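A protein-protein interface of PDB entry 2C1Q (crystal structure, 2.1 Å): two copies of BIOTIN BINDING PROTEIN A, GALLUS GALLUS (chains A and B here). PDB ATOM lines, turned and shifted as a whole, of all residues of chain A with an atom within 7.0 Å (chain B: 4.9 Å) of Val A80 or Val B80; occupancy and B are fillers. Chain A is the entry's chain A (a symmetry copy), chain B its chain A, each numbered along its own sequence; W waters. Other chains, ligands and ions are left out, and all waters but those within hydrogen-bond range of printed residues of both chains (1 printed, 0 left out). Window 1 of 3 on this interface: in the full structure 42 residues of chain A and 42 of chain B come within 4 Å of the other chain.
Phe A66 touches Thr B78 (C to CG2, 3.8 Å). Gly A67 touches Thr B78 (N to CG2, 3.9 Å). CA of Gly A67 touches CG1 of Val B80, at 3.9 Å. Thr A78 touches Gly B67. Val B80 touches Val A80. Val A80 touches Phe B81. CG2 of Val A80 touches CB of Val B82, at 3.8 Å. Val B80 touches Val A82 (CG2 to CB, 3.8 Å). Leu B100 touches Trp A99. CB of Leu A100 touches CG1 of Val B82, 3.7 Å away.
Printed residues of chain A that touch a printed residue of chain B: Phe A66, Gly A67, Phe A68, Thr A69, Thr A78, Val A80, Phe A81, Val A82, Ala A98, Trp A99, Leu A100 and Arg A102. Hydrophobic or aromatic side chains of chain A that line the printed part of chain B: Val A80, Val A82, Ala A98 and Leu A100. Along chain A the printed residues that touch a printed residue of chain B span positions 66 to 102. Of the 11 printed residues of chain B, 10 touch a printed residue of chain A. Printed residues of chain B that touch a printed residue of chain A: Gly B67, Phe B68, Thr B69, Thr B78, Val B80, Phe B81, Val B82, Ala B98, Trp B99 and Leu B100. Along chain B the printed residues that touch a printed residue of chain A span positions 67 to 100. Among the printed residues, 25 pairs touch across the chains.
O of Phe B68 sits at hydrogen-bond distance from N of Phe B81, at 2.8 Å. The backbone carbonyl oxygen of Leu B100 sits at hydrogen-bond distance from the backbone NH of Val B80, 3.0 Å away. The backbone NH (N) of Val B82 lies within hydrogen-bond range of the backbone carbonyl oxygen (O) of Ala B98 (2.8 Å). The backbone carbonyl oxygen (O) of Gly A83 lies within hydrogen-bond range of the backbone NH (N) of Phe A66 (2.8 Å). The backbone NH of Phe A81 sits at hydrogen-bond distance from the backbone carbonyl oxygen of Phe A68 (2.8 Å). N of Val A80 sits at hydrogen-bond distance from O of Leu A100 (3.0 Å).
Water W1 bridges the side-chain hydroxyl of Thr B69 (2.7 Å) and the side-chain hydroxyl of Thr A69 (2.7 Å).
O of Gly B67 lies close to OG1 of Thr A69. OG1 of Thr B69 lies close to O of Gly A67. The guanidinium group of Arg A102 lies within hydrogen-bond range of the backbone carbonyl oxygen of Val B82 (3.2 Å).
Gly A67 touches Val B80, and with the chains exchanged Val A80 touches Gly B67. Phe A68 touches Thr B69, and with the chains exchanged Thr A69 touches Phe B68. Trp A99 touches Leu B100, and with the chains exchanged Leu A100 touches Trp B99. Leu B100 touches its own counterpart, Leu A100.
Of chain B, only Gly B67 (3.9 Å), Val B80 (3.5 Å), Phe B81 (3.7 Å) and Val B82 (3.8 Å) come within 4 Å of Val A80. Val B80 touches four residues of chain A. Of the printed residues of chain B, Val A82 touches Thr B78 (3.6 Å), Val B80 (3.8 Å) and Leu B100 (3.7 Å). Printed residues of chain B within 4 Å of Ala A98: Leu B100. Printed residues of chain A within 4 Å of Thr B78: Phe A66 (3.8 Å), Gly A67 (3.9 Å) and Val A82 (3.6 Å).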
ATOM      1  N   PHE A  66      15.095   2.314 -22.896  1.00  0.00           N
ATOM      2  CA  PHE A  66      15.246   0.933 -22.444  1.00  0.00           C
ATOM      3  C   PHE A  66      16.548   0.326 -22.935  1.00  0.00           C
ATOM      4  O   PHE A  66      17.232   0.899 -23.759  1.00  0.00           O
ATOM      5  CB  PHE A  66      14.066   0.090 -22.943  1.00  0.00           C
ATOM      6  CG  PHE A  66      13.926   0.104 -24.421  1.00  0.00           C
ATOM      7  CD1 PHE A  66      14.433  -0.935 -25.190  1.00  0.00           C
ATOM      8  CD2 PHE A  66      13.343   1.191 -25.075  1.00  0.00           C
ATOM      9  CE1 PHE A  66      14.302  -0.898 -26.598  1.00  0.00           C
ATOM     10  CE2 PHE A  66      13.223   1.224 -26.471  1.00  0.00           C
ATOM     11  CZ  PHE A  66      13.712   0.176 -27.226  1.00  0.00           C
ATOM     12  N   GLY A  67      16.889  -0.845 -22.424  1.00  0.00           N
ATOM     13  CA  GLY A  67      18.061  -1.578 -22.903  1.00  0.00           C
ATOM     14  C   GLY A  67      17.825  -3.045 -22.767  1.00  0.00           C
ATOM     15  O   GLY A  67      17.014  -3.452 -21.968  1.00  0.00           O
ATOM     16  N   PHE A  68      18.518  -3.858 -23.565  1.00  0.00           N
ATOM     17  CA  PHE A  68      18.542  -5.295 -23.317  1.00  0.00           C
ATOM     18  C   PHE A  68      19.816  -5.960 -23.780  1.00  0.00           C
ATOM     19  O   PHE A  68      20.571  -5.398 -24.561  1.00  0.00           O
ATOM     20  CB  PHE A  68      17.339  -5.980 -23.963  1.00  0.00           C
ATOM     21  CG  PHE A  68      17.214  -5.757 -25.454  1.00  0.00           C
ATOM     22  CD1 PHE A  68      17.789  -6.643 -26.343  1.00  0.00           C
ATOM     23  CD2 PHE A  68      16.468  -4.691 -25.960  1.00  0.00           C
ATOM     24  CE1 PHE A  68      17.679  -6.478 -27.703  1.00  0.00           C
ATOM     25  CE2 PHE A  68      16.329  -4.532 -27.354  1.00  0.00           C
ATOM     26  CZ  PHE A  68      16.940  -5.399 -28.214  1.00  0.00           C
ATOM     27  N   THR A  69      19.999  -7.192 -23.312  1.00  0.00           N
ATOM     28  CA  THR A  69      21.134  -8.027 -23.623  1.00  0.00           C
ATOM     29  C   THR A  69      20.586  -9.218 -24.408  1.00  0.00           C
ATOM     30  O   THR A  69      19.572  -9.795 -24.035  1.00  0.00           O
ATOM     31  CB  THR A  69      21.778  -8.536 -22.311  1.00  0.00           C
ATOM     32  OG1 THR A  69      22.140  -7.414 -21.485  1.00  0.00           O
ATOM     33  CG2 THR A  69      23.003  -9.363 -22.584  1.00  0.00           C
ATOM     34  N   VAL A  70      21.216  -9.546 -25.525  1.00  0.00           N
ATOM     35  CA  VAL A  70      20.870 -10.746 -26.262  1.00  0.00           C
ATOM     36  C   VAL A  70      21.979 -11.774 -25.999  1.00  0.00           C
ATOM     37  O   VAL A  70      23.166 -11.505 -26.206  1.00  0.00           O
ATOM     38  CB  VAL A  70      20.771 -10.514 -27.792  1.00  0.00           C
ATOM     39  CG1 VAL A  70      20.376 -11.816 -28.469  1.00  0.00           C
ATOM     40  CG2 VAL A  70      19.752  -9.389 -28.122  1.00  0.00           C
ATOM     41  N   TRP A  72      23.359 -14.710 -27.463  1.00  0.00           N
ATOM     42  CA  TRP A  72      23.295 -15.454 -28.732  1.00  0.00           C
ATOM     43  C   TRP A  72      23.453 -16.951 -28.530  1.00  0.00           C
ATOM     44  O   TRP A  72      24.391 -17.392 -27.868  1.00  0.00           O
ATOM     45  CB  TRP A  72      24.326 -14.934 -29.743  1.00  0.00           C
ATOM     46  CG  TRP A  72      24.140 -13.473 -30.022  1.00  0.00           C
ATOM     47  CD1 TRP A  72      24.953 -12.455 -29.607  1.00  0.00           C
ATOM     48  CD2 TRP A  72      23.045 -12.859 -30.711  1.00  0.00           C
ATOM     49  NE1 TRP A  72      24.447 -11.248 -30.008  1.00  0.00           N
ATOM     50  CE2 TRP A  72      23.282 -11.463 -30.703  1.00  0.00           C
ATOM     51  CE3 TRP A  72      21.911 -13.354 -31.390  1.00  0.00           C
ATOM     52  CZ2 TRP A  72      22.417 -10.557 -31.298  1.00  0.00           C
ATOM     53  CZ3 TRP A  72      21.052 -12.454 -31.990  1.00  0.00           C
ATOM     54  CH2 TRP A  72      21.320 -11.054 -31.949  1.00  0.00           C
ATOM     55  N   THR A  78      28.023 -11.445 -27.267  1.00  0.00           N
ATOM     56  CA  THR A  78      26.899 -10.872 -26.563  1.00  0.00           C
ATOM     57  C   THR A  78      26.637  -9.488 -27.155  1.00  0.00           C
ATOM     58  O   THR A  78      27.569  -8.733 -27.376  1.00  0.00           O
ATOM     59  CB  THR A  78      27.177 -10.758 -25.045  1.00  0.00           C
ATOM     60  OG1 THR A  78      27.404 -12.070 -24.500  1.00  0.00           O
ATOM     61  CG2 THR A  78      26.021 -10.197 -24.360  1.00  0.00           C
ATOM     62  N   THR A  79      25.385  -9.188 -27.473  1.00  0.00           N
ATOM     63  CA  THR A  79      25.021  -7.839 -27.901  1.00  0.00           C
ATOM     64  C   THR A  79      24.164  -7.174 -26.863  1.00  0.00           C
ATOM     65  O   THR A  79      23.292  -7.817 -26.264  1.00  0.00           O
ATOM     66  CB  THR A  79      24.248  -7.802 -29.239  1.00  0.00           C
ATOM     67  OG1 THR A  79      25.030  -8.410 -30.258  1.00  0.00           O
ATOM     68  CG2 THR A  79      24.007  -6.332 -29.668  1.00  0.00           C
ATOM     69  N   VAL A  80      24.372  -5.871 -26.676  1.00  0.00           N
ATOM     70  CA  VAL A  80      23.449  -5.082 -25.868  1.00  0.00           C
ATOM     71  C   VAL A  80      22.886  -3.979 -26.724  1.00  0.00           C
ATOM     72  O   VAL A  80      23.564  -3.466 -27.566  1.00  0.00           O
ATOM     73  CB  VAL A  80      24.109  -4.481 -24.599  1.00  0.00           C
ATOM     74  CG1 VAL A  80      24.396  -5.570 -23.639  1.00  0.00           C
ATOM     75  CG2 VAL A  80      25.364  -3.669 -24.962  1.00  0.00           C
ATOM     76  N   PHE A  81      21.627  -3.638 -26.519  1.00  0.00           N
ATOM     77  CA  PHE A  81      20.978  -2.663 -27.358  1.00  0.00           C
ATOM     78  C   PHE A  81      20.427  -1.643 -26.383  1.00  0.00           C
ATOM     79  O   PHE A  81      19.921  -2.004 -25.329  1.00  0.00           O
ATOM     80  CB  PHE A  81      19.792  -3.285 -28.033  1.00  0.00           C
ATOM     81  CG  PHE A  81      20.096  -4.108 -29.242  1.00  0.00           C
ATOM     82  CD1 PHE A  81      19.890  -3.571 -30.530  1.00  0.00           C
ATOM     83  CD2 PHE A  81      20.480  -5.451 -29.114  1.00  0.00           C
ATOM     84  CE1 PHE A  81      20.123  -4.349 -31.689  1.00  0.00           C
ATOM     85  CE2 PHE A  81      20.708  -6.245 -30.251  1.00  0.00           C
ATOM     86  CZ  PHE A  81      20.525  -5.696 -31.556  1.00  0.00           C
ATOM     87  N   VAL A  82      20.486  -0.381 -26.741  1.00  0.00           N
ATOM     88  CA  VAL A  82      19.898   0.646 -25.911  1.00  0.00           C
ATOM     89  C   VAL A  82      19.097   1.614 -26.834  1.00  0.00           C
ATOM     90  O   VAL A  82      19.506   1.886 -27.985  1.00  0.00           O
ATOM     91  CB  VAL A  82      20.992   1.286 -25.004  1.00  0.00           C
ATOM     92  CG1 VAL A  82      21.987   2.143 -25.822  1.00  0.00           C
ATOM     93  CG2 VAL A  82      20.386   2.065 -23.835  1.00  0.00           C
ATOM     94  N   GLY A  83      17.927   2.073 -26.365  1.00  0.00           N
ATOM     95  CA  GLY A  83      17.022   2.802 -27.227  1.00  0.00           C
ATOM     96  C   GLY A  83      15.860   3.524 -26.582  1.00  0.00           C
ATOM     97  O   GLY A  83      15.738   3.550 -25.366  1.00  0.00           O
ATOM     98  N   MET A  97      17.705   2.560 -31.781  1.00  0.00           N
ATOM     99  CA  MET A  97      18.594   1.755 -30.946  1.00  0.00           C
ATOM    100  C   MET A  97      20.037   1.895 -31.362  1.00  0.00           C
ATOM    101  O   MET A  97      20.328   2.131 -32.512  1.00  0.00           O
ATOM    102  CB  MET A  97      18.199   0.284 -30.956  1.00  0.00           C
ATOM    103  CG  MET A  97      16.789   0.052 -30.406  1.00  0.00           C
ATOM    104  SD  MET A  97      16.508  -1.478 -29.551  1.00  0.00           S
ATOM    105  CE  MET A  97      17.029  -0.986 -27.861  1.00  0.00           C
ATOM    106  N   ALA A  98      20.927   1.816 -30.383  1.00  0.00           N
ATOM    107  CA  ALA A  98      22.353   1.765 -30.621  1.00  0.00           C
ATOM    108  C   ALA A  98      22.748   0.504 -29.897  1.00  0.00           C
ATOM    109  O   ALA A  98      22.067   0.085 -28.943  1.00  0.00           O
ATOM    110  CB  ALA A  98      23.072   3.007 -30.025  1.00  0.00           C
ATOM    111  N   TRP A  99      23.810  -0.137 -30.379  1.00  0.00           N
ATOM    112  CA  TRP A  99      24.187  -1.446 -29.875  1.00  0.00           C
ATOM    113  C   TRP A  99      25.686  -1.650 -29.868  1.00  0.00           C
ATOM    114  O   TRP A  99      26.422  -0.970 -30.571  1.00  0.00           O
ATOM    115  CB  TRP A  99      23.498  -2.562 -30.689  1.00  0.00           C
ATOM    116  CG  TRP A  99      23.763  -2.555 -32.190  1.00  0.00           C
ATOM    117  CD1 TRP A  99      22.881  -2.152 -33.170  1.00  0.00           C
ATOM    118  CD2 TRP A  99      24.954  -3.027 -32.891  1.00  0.00           C
ATOM    119  NE1 TRP A  99      23.464  -2.323 -34.422  1.00  0.00           N
ATOM    120  CE2 TRP A  99      24.724  -2.851 -34.275  1.00  0.00           C
ATOM    121  CE3 TRP A  99      26.193  -3.570 -32.473  1.00  0.00           C
ATOM    122  CZ2 TRP A  99      25.680  -3.179 -35.241  1.00  0.00           C
ATOM    123  CZ3 TRP A  99      27.123  -3.927 -33.433  1.00  0.00           C
ATOM    124  CH2 TRP A  99      26.874  -3.720 -34.801  1.00  0.00           C
ATOM    125  N   LEU A 100      26.122  -2.587 -29.035  1.00  0.00           N
ATOM    126  CA  LEU A 100      27.516  -3.027 -28.993  1.00  0.00           C
ATOM    127  C   LEU A 100      27.514  -4.534 -29.071  1.00  0.00           C
ATOM    128  O   LEU A 100      26.806  -5.192 -28.316  1.00  0.00           O
ATOM    129  CB  LEU A 100      28.203  -2.623 -27.689  1.00  0.00           C
ATOM    130  CG  LEU A 100      28.348  -1.128 -27.362  1.00  0.00           C
ATOM    131  CD1 LEU A 100      28.798  -0.951 -25.904  1.00  0.00           C
ATOM    132  CD2 LEU A 100      29.288  -0.408 -28.305  1.00  0.00           C
ATOM    133  N   LEU A 101      28.300  -5.075 -29.981  1.00  0.00           N
ATOM    134  CA  LEU A 101      28.422  -6.520 -30.113  1.00  0.00           C
ATOM    135  C   LEU A 101      29.797  -6.876 -29.604  1.00  0.00           C
ATOM    136  O   LEU A 101      30.790  -6.398 -30.133  1.00  0.00           O
ATOM    137  CB  LEU A 101      28.269  -6.932 -31.568  1.00  0.00           C
ATOM    138  CG  LEU A 101      28.743  -8.334 -32.019  1.00  0.00           C
ATOM    139  CD1 LEU A 101      28.113  -9.450 -31.215  1.00  0.00           C
ATOM    140  CD2 LEU A 101      28.373  -8.530 -33.510  1.00  0.00           C
ATOM    141  N   ARG A 102      29.850  -7.744 -28.601  1.00  0.00           N
ATOM    142  CA  ARG A 102      31.109  -8.098 -27.935  1.00  0.00           C
ATOM    143  C   ARG A 102      31.460  -9.532 -28.262  1.00  0.00           C
ATOM    144  O   ARG A 102      30.735 -10.439 -27.865  1.00  0.00           O
ATOM    145  CB  ARG A 102      30.956  -7.995 -26.424  1.00  0.00           C
ATOM    146  CG  ARG A 102      32.218  -8.392 -25.599  1.00  0.00           C
ATOM    147  CD  ARG A 102      32.980  -7.179 -25.490  1.00  0.00           C
ATOM    148  NE  ARG A 102      34.209  -7.216 -24.716  1.00  0.00           N
ATOM    149  CZ  ARG A 102      34.653  -6.116 -24.125  1.00  0.00           C
ATOM    150  NH1 ARG A 102      33.910  -4.997 -24.194  1.00  0.00           N
ATOM    151  NH2 ARG A 102      35.783  -6.122 -23.464  1.00  0.00           N
ATOM    152  N   GLY B  67      26.454  -9.192 -20.641  1.00  0.00           N
ATOM    153  CA  GLY B  67      25.953  -7.827 -20.799  1.00  0.00           C
ATOM    154  C   GLY B  67      24.936  -7.541 -19.745  1.00  0.00           C
ATOM    155  O   GLY B  67      24.347  -8.454 -19.213  1.00  0.00           O
ATOM    156  N   PHE B  68      24.734  -6.265 -19.413  1.00  0.00           N
ATOM    157  CA  PHE B  68      23.588  -5.886 -18.595  1.00  0.00           C
ATOM    158  C   PHE B  68      23.092  -4.487 -18.872  1.00  0.00           C
ATOM    159  O   PHE B  68      23.789  -3.680 -19.472  1.00  0.00           O
ATOM    160  CB  PHE B  68      23.906  -6.035 -17.108  1.00  0.00           C
ATOM    161  CG  PHE B  68      25.108  -5.243 -16.641  1.00  0.00           C
ATOM    162  CD1 PHE B  68      24.952  -3.962 -16.150  1.00  0.00           C
ATOM    163  CD2 PHE B  68      26.384  -5.809 -16.639  1.00  0.00           C
ATOM    164  CE1 PHE B  68      26.020  -3.223 -15.701  1.00  0.00           C
ATOM    165  CE2 PHE B  68      27.480  -5.067 -16.154  1.00  0.00           C
ATOM    166  CZ  PHE B  68      27.307  -3.787 -15.710  1.00  0.00           C
ATOM    167  N   THR B  69      21.890  -4.216 -18.371  1.00  0.00           N
ATOM    168  CA  THR B  69      21.216  -2.946 -18.498  1.00  0.00           C
ATOM    169  C   THR B  69      21.102  -2.380 -17.084  1.00  0.00           C
ATOM    170  O   THR B  69      20.746  -3.094 -16.154  1.00  0.00           O
ATOM    171  CB  THR B  69      19.796  -3.169 -19.073  1.00  0.00           C
ATOM    172  OG1 THR B  69      19.888  -3.862 -20.331  1.00  0.00           O
ATOM    173  CG2 THR B  69      19.076  -1.866 -19.280  1.00  0.00           C
ATOM    174  N   THR B  78      19.435   5.286 -19.710  1.00  0.00           N
ATOM    175  CA  THR B  78      19.661   3.868 -19.560  1.00  0.00           C
ATOM    176  C   THR B  78      21.072   3.567 -20.061  1.00  0.00           C
ATOM    177  O   THR B  78      21.469   4.065 -21.102  1.00  0.00           O
ATOM    178  CB  THR B  78      18.626   3.039 -20.358  1.00  0.00           C
ATOM    179  OG1 THR B  78      17.304   3.319 -19.862  1.00  0.00           O
ATOM    180  CG2 THR B  78      18.866   1.615 -20.173  1.00  0.00           C
ATOM    181  N   THR B  79      21.847   2.817 -19.289  1.00  0.00           N
ATOM    182  CA  THR B  79      23.152   2.356 -19.756  1.00  0.00           C
ATOM    183  C   THR B  79      23.138   0.869 -19.966  1.00  0.00           C
ATOM    184  O   THR B  79      22.544   0.130 -19.171  1.00  0.00           O
ATOM    185  CB  THR B  79      24.308   2.679 -18.782  1.00  0.00           C
ATOM    186  OG1 THR B  79      24.370   4.083 -18.565  1.00  0.00           O
ATOM    187  CG2 THR B  79      25.661   2.257 -19.410  1.00  0.00           C
ATOM    188  N   VAL B  80      23.832   0.416 -21.009  1.00  0.00           N
ATOM    189  CA  VAL B  80      24.076  -1.012 -21.173  1.00  0.00           C
ATOM    190  C   VAL B  80      25.564  -1.244 -21.196  1.00  0.00           C
ATOM    191  O   VAL B  80      26.291  -0.432 -21.690  1.00  0.00           O
ATOM    192  CB  VAL B  80      23.431  -1.600 -22.455  1.00  0.00           C
ATOM    193  CG1 VAL B  80      21.960  -1.626 -22.291  1.00  0.00           C
ATOM    194  CG2 VAL B  80      23.870  -0.815 -23.703  1.00  0.00           C
ATOM    195  N   PHE B  81      26.011  -2.349 -20.629  1.00  0.00           N
ATOM    196  CA  PHE B  81      27.425  -2.604 -20.517  1.00  0.00           C
ATOM    197  C   PHE B  81      27.606  -3.972 -21.141  1.00  0.00           C
ATOM    198  O   PHE B  81      26.789  -4.859 -20.936  1.00  0.00           O
ATOM    199  CB  PHE B  81      27.801  -2.746 -19.072  1.00  0.00           C
ATOM    200  CG  PHE B  81      27.983  -1.465 -18.325  1.00  0.00           C
ATOM    201  CD1 PHE B  81      29.280  -0.972 -18.075  1.00  0.00           C
ATOM    202  CD2 PHE B  81      26.880  -0.800 -17.769  1.00  0.00           C
ATOM    203  CE1 PHE B  81      29.478   0.212 -17.325  1.00  0.00           C
ATOM    204  CE2 PHE B  81      27.053   0.373 -17.013  1.00  0.00           C
ATOM    205  CZ  PHE B  81      28.364   0.887 -16.781  1.00  0.00           C
ATOM    206  N   VAL B  82      28.686  -4.162 -21.865  1.00  0.00           N
ATOM    207  CA  VAL B  82      28.981  -5.465 -22.416  1.00  0.00           C
ATOM    208  C   VAL B  82      30.490  -5.764 -22.167  1.00  0.00           C
ATOM    209  O   VAL B  82      31.341  -4.849 -22.214  1.00  0.00           O
ATOM    210  CB  VAL B  82      28.485  -5.541 -23.892  1.00  0.00           C
ATOM    211  CG1 VAL B  82      29.337  -4.655 -24.831  1.00  0.00           C
ATOM    212  CG2 VAL B  82      28.387  -6.983 -24.392  1.00  0.00           C
ATOM    213  N   ALA B  98      32.523  -2.325 -22.290  1.00  0.00           N
ATOM    214  CA  ALA B  98      32.247  -1.190 -23.144  1.00  0.00           C
ATOM    215  C   ALA B  98      30.790  -0.930 -22.859  1.00  0.00           C
ATOM    216  O   ALA B  98      30.051  -1.850 -22.464  1.00  0.00           O
ATOM    217  CB  ALA B  98      32.475  -1.539 -24.642  1.00  0.00           C
ATOM    218  N   TRP B  99      30.384   0.329 -23.001  1.00  0.00           N
ATOM    219  CA  TRP B  99      29.051   0.736 -22.595  1.00  0.00           C
ATOM    220  C   TRP B  99      28.482   1.818 -23.488  1.00  0.00           C
ATOM    221  O   TRP B  99      29.211   2.519 -24.177  1.00  0.00           O
ATOM    222  CB  TRP B  99      29.046   1.199 -21.123  1.00  0.00           C
ATOM    223  CG  TRP B  99      29.997   2.339 -20.778  1.00  0.00           C
ATOM    224  CD1 TRP B  99      31.187   2.225 -20.091  1.00  0.00           C
ATOM    225  CD2 TRP B  99      29.818   3.764 -21.039  1.00  0.00           C
ATOM    226  NE1 TRP B  99      31.759   3.486 -19.936  1.00  0.00           N
ATOM    227  CE2 TRP B  99      30.945   4.433 -20.507  1.00  0.00           C
ATOM    228  CE3 TRP B  99      28.816   4.530 -21.681  1.00  0.00           C
ATOM    229  CZ2 TRP B  99      31.109   5.819 -20.607  1.00  0.00           C
ATOM    230  CZ3 TRP B  99      28.964   5.903 -21.747  1.00  0.00           C
ATOM    231  CH2 TRP B  99      30.106   6.539 -21.228  1.00  0.00           C
ATOM    232  N   LEU B 100      27.158   1.918 -23.477  1.00  0.00           N
ATOM    233  CA  LEU B 100      26.437   2.992 -24.158  1.00  0.00           C
ATOM    234  C   LEU B 100      25.474   3.588 -23.162  1.00  0.00           C
ATOM    235  O   LEU B 100      24.716   2.866 -22.524  1.00  0.00           O
ATOM    236  CB  LEU B 100      25.627   2.472 -25.345  1.00  0.00           C
ATOM    237  CG  LEU B 100      26.373   1.817 -26.519  1.00  0.00           C
ATOM    238  CD1 LEU B 100      25.372   1.121 -27.453  1.00  0.00           C
ATOM    239  CD2 LEU B 100      27.234   2.795 -27.289  1.00  0.00           C
HETATM  240  O   HOH W   1      20.058  -6.540 -19.998  1.00  0.00           O
